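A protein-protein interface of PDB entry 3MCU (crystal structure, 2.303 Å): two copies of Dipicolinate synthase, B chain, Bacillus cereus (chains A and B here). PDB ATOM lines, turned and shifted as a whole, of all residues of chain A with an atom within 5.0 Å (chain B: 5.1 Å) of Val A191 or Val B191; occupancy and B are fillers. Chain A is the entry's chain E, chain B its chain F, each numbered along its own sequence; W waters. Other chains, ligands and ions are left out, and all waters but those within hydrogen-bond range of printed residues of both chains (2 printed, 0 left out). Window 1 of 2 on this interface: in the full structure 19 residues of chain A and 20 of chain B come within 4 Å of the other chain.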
ATOM      1  N   LEU A 134      15.308  -5.667   4.561  1.00  0.00           N
ATOM      2  CA  LEU A 134      14.586  -6.825   4.074  1.00  0.00           C
ATOM      3  C   LEU A 134      14.550  -6.732   2.545  1.00  0.00           C
ATOM      4  O   LEU A 134      13.898  -7.523   1.867  1.00  0.00           O
ATOM      5  CB  LEU A 134      13.174  -6.850   4.659  1.00  0.00           C
ATOM      6  CG  LEU A 134      13.105  -7.093   6.176  1.00  0.00           C
ATOM      7  CD1 LEU A 134      11.663  -7.011   6.687  1.00  0.00           C
ATOM      8  CD2 LEU A 134      13.729  -8.441   6.535  1.00  0.00           C
ATOM      9  N   PHE A 155      17.023  -6.662  16.871  1.00  0.00           N
ATOM     10  CA  PHE A 155      16.476  -5.727  15.902  1.00  0.00           C
ATOM     11  C   PHE A 155      15.213  -6.279  15.269  1.00  0.00           C
ATOM     12  O   PHE A 155      14.910  -7.466  15.399  1.00  0.00           O
ATOM     13  CB  PHE A 155      17.504  -5.470  14.809  1.00  0.00           C
ATOM     14  CG  PHE A 155      17.860  -6.702  14.026  1.00  0.00           C
ATOM     15  CD1 PHE A 155      17.104  -7.083  12.920  1.00  0.00           C
ATOM     16  CD2 PHE A 155      18.945  -7.482  14.392  1.00  0.00           C
ATOM     17  CE1 PHE A 155      17.440  -8.230  12.187  1.00  0.00           C
ATOM     18  CE2 PHE A 155      19.285  -8.627  13.674  1.00  0.00           C
ATOM     19  CZ  PHE A 155      18.539  -9.005  12.572  1.00  0.00           C
ATOM     20  N   GLY A 156      14.497  -5.415  14.551  1.00  0.00           N
ATOM     21  CA  GLY A 156      13.293  -5.816  13.836  1.00  0.00           C
ATOM     22  C   GLY A 156      12.726  -4.689  12.994  1.00  0.00           C
ATOM     23  O   GLY A 156      13.347  -3.642  12.859  1.00  0.00           O
ATOM     24  N   GLN A 157      11.549  -4.908  12.418  1.00  0.00           N
ATOM     25  CA  GLN A 157      10.869  -3.853  11.661  1.00  0.00           C
ATOM     26  C   GLN A 157      10.414  -2.735  12.597  1.00  0.00           C
ATOM     27  O   GLN A 157       9.716  -2.991  13.560  1.00  0.00           O
ATOM     28  CB  GLN A 157       9.666  -4.433  10.909  1.00  0.00           C
ATOM     29  CG  GLN A 157      10.037  -5.450   9.860  1.00  0.00           C
ATOM     30  CD  GLN A 157       8.845  -6.002   9.114  1.00  0.00           C
ATOM     31  OE1 GLN A 157       8.186  -6.924   9.581  1.00  0.00           O
ATOM     32  NE2 GLN A 157       8.564  -5.441   7.938  1.00  0.00           N
ATOM     33  N   MET A 167      14.601  -2.321   8.947  1.00  0.00           N
ATOM     34  CA  MET A 167      14.900  -2.919  10.259  1.00  0.00           C
ATOM     35  C   MET A 167      15.919  -2.099  11.029  1.00  0.00           C
ATOM     36  O   MET A 167      16.889  -1.562  10.464  1.00  0.00           O
ATOM     37  CB  MET A 167      15.313  -4.393  10.168  1.00  0.00           C
ATOM     38  CG  MET A 167      14.157  -5.295   9.767  1.00  0.00           C
ATOM     39  SD  MET A 167      14.417  -7.223   9.979  1.00  0.00           S
ATOM     40  CE  MET A 167      16.152  -7.467   9.073  1.00  0.00           C
ATOM     41  N   PRO A 189      16.330 -12.877  22.679  1.00  0.00           N
ATOM     42  CA  PRO A 189      16.075 -13.071  21.240  1.00  0.00           C
ATOM     43  C   PRO A 189      16.697 -11.954  20.405  1.00  0.00           C
ATOM     44  O   PRO A 189      16.713 -10.810  20.841  1.00  0.00           O
ATOM     45  CB  PRO A 189      14.537 -13.039  21.134  1.00  0.00           C
ATOM     46  CG  PRO A 189      14.067 -12.325  22.382  1.00  0.00           C
ATOM     47  CD  PRO A 189      15.108 -12.542  23.444  1.00  0.00           C
ATOM     48  N   VAL A 190      17.232 -12.293  19.238  1.00  0.00           N
ATOM     49  CA  VAL A 190      17.908 -11.308  18.414  1.00  0.00           C
ATOM     50  C   VAL A 190      16.929 -10.742  17.362  1.00  0.00           C
ATOM     51  O   VAL A 190      17.103  -9.632  16.852  1.00  0.00           O
ATOM     52  CB  VAL A 190      19.225 -11.896  17.814  1.00  0.00           C
ATOM     53  CG1 VAL A 190      18.934 -13.066  16.880  1.00  0.00           C
ATOM     54  CG2 VAL A 190      20.047 -10.822  17.126  1.00  0.00           C
ATOM     55  N   VAL A 191      15.871 -11.494  17.087  1.00  0.00           N
ATOM     56  CA  VAL A 191      14.822 -11.030  16.205  1.00  0.00           C
ATOM     57  C   VAL A 191      13.573 -10.634  16.995  1.00  0.00           C
ATOM     58  O   VAL A 191      12.882 -11.491  17.550  1.00  0.00           O
ATOM     59  CB  VAL A 191      14.454 -12.113  15.175  1.00  0.00           C
ATOM     60  CG1 VAL A 191      13.445 -11.568  14.177  1.00  0.00           C
ATOM     61  CG2 VAL A 191      15.720 -12.611  14.451  1.00  0.00           C
ATOM     62  N   VAL A 192      13.278  -9.337  17.038  1.00  0.00           N
ATOM     63  CA  VAL A 192      12.168  -8.857  17.851  1.00  0.00           C
ATOM     64  C   VAL A 192      11.231  -7.929  17.070  1.00  0.00           C
ATOM     65  O   VAL A 192      11.521  -7.508  15.953  1.00  0.00           O
ATOM     66  CB  VAL A 192      12.672  -8.129  19.117  1.00  0.00           C
ATOM     67  CG1 VAL A 192      13.434  -9.092  20.012  1.00  0.00           C
ATOM     68  CG2 VAL A 192      13.564  -6.964  18.730  1.00  0.00           C
ATOM     69  N   GLU A 193      10.094  -7.630  17.673  1.00  0.00           N
ATOM     70  CA  GLU A 193       9.162  -6.700  17.084  1.00  0.00           C
ATOM     71  C   GLU A 193       9.529  -5.295  17.505  1.00  0.00           C
ATOM     72  O   GLU A 193       8.920  -4.715  18.395  1.00  0.00           O
ATOM     73  CB  GLU A 193       7.732  -7.066  17.460  1.00  0.00           C
ATOM     74  CG  GLU A 193       7.289  -8.367  16.807  1.00  0.00           C
ATOM     75  CD  GLU A 193       6.011  -8.924  17.395  1.00  0.00           C
ATOM     76  OE1 GLU A 193       5.457  -8.294  18.316  1.00  0.00           O
ATOM     77  OE2 GLU A 193       5.568  -9.999  16.939  1.00  0.00           O
ATOM     78  N   PHE A 195       8.768  -2.666  16.271  1.00  0.00           N
ATOM     79  CA  PHE A 195       7.658  -1.721  16.141  1.00  0.00           C
ATOM     80  C   PHE A 195       6.868  -1.535  17.443  1.00  0.00           C
ATOM     81  O   PHE A 195       6.228  -0.505  17.635  1.00  0.00           O
ATOM     82  CB  PHE A 195       6.728  -2.053  14.951  1.00  0.00           C
ATOM     83  CG  PHE A 195       6.135  -3.436  14.992  1.00  0.00           C
ATOM     84  CD1 PHE A 195       4.907  -3.667  15.605  1.00  0.00           C
ATOM     85  CD2 PHE A 195       6.804  -4.511  14.414  1.00  0.00           C
ATOM     86  CE1 PHE A 195       4.354  -4.947  15.644  1.00  0.00           C
ATOM     87  CE2 PHE A 195       6.259  -5.798  14.443  1.00  0.00           C
ATOM     88  CZ  PHE A 195       5.029  -6.013  15.061  1.00  0.00           C
ATOM     89  N   LEU B 134      19.124 -18.479  10.927  1.00  0.00           N
ATOM     90  CA  LEU B 134      20.027 -17.401  11.312  1.00  0.00           C
ATOM     91  C   LEU B 134      21.482 -17.845  11.236  1.00  0.00           C
ATOM     92  O   LEU B 134      22.388 -17.126  11.669  1.00  0.00           O
ATOM     93  CB  LEU B 134      19.682 -16.877  12.710  1.00  0.00           C
ATOM     94  CG  LEU B 134      18.311 -16.210  12.814  1.00  0.00           C
ATOM     95  CD1 LEU B 134      17.969 -15.956  14.271  1.00  0.00           C
ATOM     96  CD2 LEU B 134      18.287 -14.911  12.023  1.00  0.00           C
ATOM     97  N   PHE B 155       7.241 -14.705  10.075  1.00  0.00           N
ATOM     98  CA  PHE B 155       8.067 -15.696  10.716  1.00  0.00           C
ATOM     99  C   PHE B 155       8.950 -14.987  11.728  1.00  0.00           C
ATOM    100  O   PHE B 155       9.065 -13.762  11.705  1.00  0.00           O
ATOM    101  CB  PHE B 155       8.927 -16.403   9.666  1.00  0.00           C
ATOM    102  CG  PHE B 155       9.875 -15.472   8.942  1.00  0.00           C
ATOM    103  CD1 PHE B 155      11.151 -15.240   9.439  1.00  0.00           C
ATOM    104  CD2 PHE B 155       9.485 -14.818   7.788  1.00  0.00           C
ATOM    105  CE1 PHE B 155      12.025 -14.383   8.797  1.00  0.00           C
ATOM    106  CE2 PHE B 155      10.360 -13.950   7.127  1.00  0.00           C
ATOM    107  CZ  PHE B 155      11.632 -13.732   7.638  1.00  0.00           C
ATOM    108  N   GLY B 156       9.548 -15.768  12.616  1.00  0.00           N
ATOM    109  CA  GLY B 156      10.535 -15.285  13.562  1.00  0.00           C
ATOM    110  C   GLY B 156      11.096 -16.440  14.382  1.00  0.00           C
ATOM    111  O   GLY B 156      10.880 -17.614  14.064  1.00  0.00           O
ATOM    112  N   GLN B 157      11.809 -16.107  15.449  1.00  0.00           N
ATOM    113  CA  GLN B 157      12.376 -17.114  16.353  1.00  0.00           C
ATOM    114  C   GLN B 157      11.295 -17.871  17.141  1.00  0.00           C
ATOM    115  O   GLN B 157      10.493 -17.258  17.844  1.00  0.00           O
ATOM    116  CB  GLN B 157      13.395 -16.461  17.297  1.00  0.00           C
ATOM    117  CG  GLN B 157      14.629 -15.950  16.564  1.00  0.00           C
ATOM    118  CD  GLN B 157      15.702 -15.403  17.483  1.00  0.00           C
ATOM    119  OE1 GLN B 157      15.638 -14.248  17.914  1.00  0.00           O
ATOM    120  NE2 GLN B 157      16.710 -16.228  17.777  1.00  0.00           N
ATOM    121  N   MET B 167      14.162 -20.248  12.806  1.00  0.00           N
ATOM    122  CA  MET B 167      12.999 -19.427  12.488  1.00  0.00           C
ATOM    123  C   MET B 167      11.905 -20.246  11.820  1.00  0.00           C
ATOM    124  O   MET B 167      12.188 -21.157  11.033  1.00  0.00           O
ATOM    125  CB  MET B 167      13.370 -18.177  11.696  1.00  0.00           C
ATOM    126  CG  MET B 167      14.191 -17.201  12.540  1.00  0.00           C
ATOM    127  SD  MET B 167      14.277 -15.382  11.838  1.00  0.00           S
ATOM    128  CE  MET B 167      14.920 -15.786  10.040  1.00  0.00           C
ATOM    129  N   PRO B 189       3.137  -7.217   9.650  1.00  0.00           N
ATOM    130  CA  PRO B 189       4.608  -7.326   9.725  1.00  0.00           C
ATOM    131  C   PRO B 189       5.087  -8.700   9.274  1.00  0.00           C
ATOM    132  O   PRO B 189       4.437  -9.691   9.575  1.00  0.00           O
ATOM    133  CB  PRO B 189       4.903  -7.132  11.217  1.00  0.00           C
ATOM    134  CG  PRO B 189       3.605  -7.486  11.932  1.00  0.00           C
ATOM    135  CD  PRO B 189       2.488  -7.198  10.979  1.00  0.00           C
ATOM    136  N   VAL B 190       6.194  -8.767   8.549  1.00  0.00           N
ATOM    137  CA  VAL B 190       6.700 -10.050   8.091  1.00  0.00           C
ATOM    138  C   VAL B 190       7.678 -10.644   9.100  1.00  0.00           C
ATOM    139  O   VAL B 190       7.899 -11.854   9.112  1.00  0.00           O
ATOM    140  CB  VAL B 190       7.371  -9.964   6.687  1.00  0.00           C
ATOM    141  CG1 VAL B 190       8.794  -9.444   6.798  1.00  0.00           C
ATOM    142  CG2 VAL B 190       7.387 -11.328   6.030  1.00  0.00           C
ATOM    143  N   VAL B 191       8.264  -9.791   9.934  1.00  0.00           N
ATOM    144  CA  VAL B 191       9.174 -10.251  10.980  1.00  0.00           C
ATOM    145  C   VAL B 191       8.512 -10.114  12.350  1.00  0.00           C
ATOM    146  O   VAL B 191       8.238  -9.003  12.815  1.00  0.00           O
ATOM    147  CB  VAL B 191      10.529  -9.486  10.960  1.00  0.00           C
ATOM    148  CG1 VAL B 191      11.401  -9.934  12.102  1.00  0.00           C
ATOM    149  CG2 VAL B 191      11.260  -9.705   9.628  1.00  0.00           C
ATOM    150  N   VAL B 192       8.255 -11.249  12.990  1.00  0.00           N
ATOM    151  CA  VAL B 192       7.490 -11.243  14.214  1.00  0.00           C
ATOM    152  C   VAL B 192       8.099 -12.095  15.329  1.00  0.00           C
ATOM    153  O   VAL B 192       8.936 -12.961  15.091  1.00  0.00           O
ATOM    154  CB  VAL B 192       6.028 -11.700  13.962  1.00  0.00           C
ATOM    155  CG1 VAL B 192       5.355 -10.797  12.941  1.00  0.00           C
ATOM    156  CG2 VAL B 192       5.989 -13.165  13.527  1.00  0.00           C
ATOM    157  N   GLU B 193       7.664 -11.841  16.554  1.00  0.00           N
ATOM    158  CA  GLU B 193       8.121 -12.640  17.674  1.00  0.00           C
ATOM    159  C   GLU B 193       7.352 -13.956  17.716  1.00  0.00           C
ATOM    160  O   GLU B 193       6.380 -14.109  18.449  1.00  0.00           O
ATOM    161  CB  GLU B 193       8.006 -11.854  18.979  1.00  0.00           C
ATOM    162  CG  GLU B 193       9.087 -10.786  19.111  1.00  0.00           C
ATOM    163  CD  GLU B 193       8.768  -9.740  20.171  1.00  0.00           C
ATOM    164  OE1 GLU B 193       9.552  -8.780  20.338  1.00  0.00           O
ATOM    165  OE2 GLU B 193       7.719  -9.871  20.826  1.00  0.00           O
ATOM    166  N   PHE B 195       7.978 -16.749  18.988  1.00  0.00           N
ATOM    167  CA  PHE B 195       8.023 -17.460  20.258  1.00  0.00           C
ATOM    168  C   PHE B 195       6.842 -17.097  21.156  1.00  0.00           C
ATOM    169  O   PHE B 195       6.578 -17.789  22.137  1.00  0.00           O
ATOM    170  CB  PHE B 195       9.354 -17.222  20.994  1.00  0.00           C
ATOM    171  CG  PHE B 195       9.703 -15.770  21.174  1.00  0.00           C
ATOM    172  CD1 PHE B 195       9.300 -15.079  22.307  1.00  0.00           C
ATOM    173  CD2 PHE B 195      10.443 -15.093  20.212  1.00  0.00           C
ATOM    174  CE1 PHE B 195       9.625 -13.746  22.476  1.00  0.00           C
ATOM    175  CE2 PHE B 195      10.772 -13.759  20.380  1.00  0.00           C
ATOM    176  CZ  PHE B 195      10.360 -13.085  21.519  1.00  0.00           C
HETATM  177  O   HOH W   1       9.732  -6.988  13.554  1.00  0.00           O
HETATM  178  O   HOH W   2      11.476 -13.554  16.662  1.00  0.00           O
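OE1 of Gln A157 lies within hydrogen-bond range of N of Val B190, at 2.9 Å.
N of Val B191 lies within hydrogen-bond range of OE1 of Gln A157 (2.9 Å).
OE1 of Gln B157 is in hydrogen-bond range of N of Val A190 (2.8 Å).
The backbone NH (N) of Val A191 lies within hydrogen-bond range of the side-chain amide oxygen (OE1) of Gln B157 (2.9 Å).
OE2 of Glu A193 lies within hydrogen-bond range of N of Glu B193.
N of Phe A155 lies within hydrogen-bond range of O of Val A190 (3.0 Å).
O of Phe A155 is in hydrogen-bond range of N of Val A192, at 3.0 Å.
The backbone NH (N) of Phe A195 sits at hydrogen-bond distance from the backbone carbonyl oxygen (O) of Gln A157 (2.9 Å).
The backbone NH of Phe B155 is in hydrogen-bond range of the backbone carbonyl oxygen of Val B190 (3.1 Å).
The backbone NH of Val B192 lies within hydrogen-bond range of the backbone carbonyl oxygen of Phe B155 (2.9 Å).
N of Phe B195 is in hydrogen-bond range of O of Gln B157, at 2.8 Å.
Among the printed residues, merely in contact across the chains: Leu A134 with Val B190 (3.8 Å), Gln A157 with Pro B189 (3.6 Å), Pro A189 with Gln B157 (3.5 Å), Pro A189 with Phe B195 (3.9 Å), Val A191 with Val B191 (3.3 Å), Val A192 with Glu B193 (3.4 Å), Glu A193 with Val B192 (3.5 Å) and Phe A195 with Pro B189 (3.7 Å).
Printed residues of chain B within 4 Å of Val A191: Gln B157 and Val B191.
Printed residues of chain A within 4 Å of Val B191: Gln A157 and Val A191.
Of the printed residues of chain B, Leu A134 touches Val B190.
Of the printed residues of chain A, Val B190 touches Leu A134 and Gln A157.
Of the printed residues of chain A, Gln B157 touches Pro A189 (3.5 Å), Val A190 (2.8 Å) and Val A191 (2.9 Å).
Phe B155 touches none of the printed residues of chain A.
Phe A155 touches none of the printed residues of chain B.
The nearest printed residue of chain A that does not touch Val B191 is Leu A134 (4.01 Å).
The nearest printed residue of chain B that does not touch Gln A157 is Val B192 (5.5 Å).
Of the 11 printed residues of chain B, 7 touch a printed residue of chain A.
Of the 11 printed residues of chain A, 8 touch a printed residue of chain B.
Hydrophobic or aromatic side chains of chain A within 4 Å of the printed part of chain B: Leu A134, Pro A189, Val A190, Val A191, Val A192 and Phe A195.
Among the printed residues, 13 pairs touch across the chains.
Among the printed residues, no Asp or Glu carboxylate lies within 4 Å of a Lys or Arg side-chain nitrogen of the other chain.
Gln A157 touches Pro B189, and with the chains exchanged Pro A189 touches Gln B157.
Gln A157 touches Val B191, and with the chains exchanged Val A191 touches Gln B157.
Pro A189 touches Phe B195, and with the chains exchanged Phe A195 touches Pro B189.
Glu B193 touches its own counterpart, Glu A193.
Positions printed for both chains: 134, 155, 156, 157, 167, 189, 190, 191, 192, 193 and 195.
Water W1 lies within hydrogen-bond range of O of Val B191 (2.6 Å), N of Gln A157 (3.0 Å) and O of Val A192 (3.0 Å).
Water W2 lies within hydrogen-bond range of the backbone carbonyl oxygen of Val A191 (2.6 Å), the backbone NH of Gln B157 (2.8 Å) and the backbone carbonyl oxygen of Val B192 (3.0 Å).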
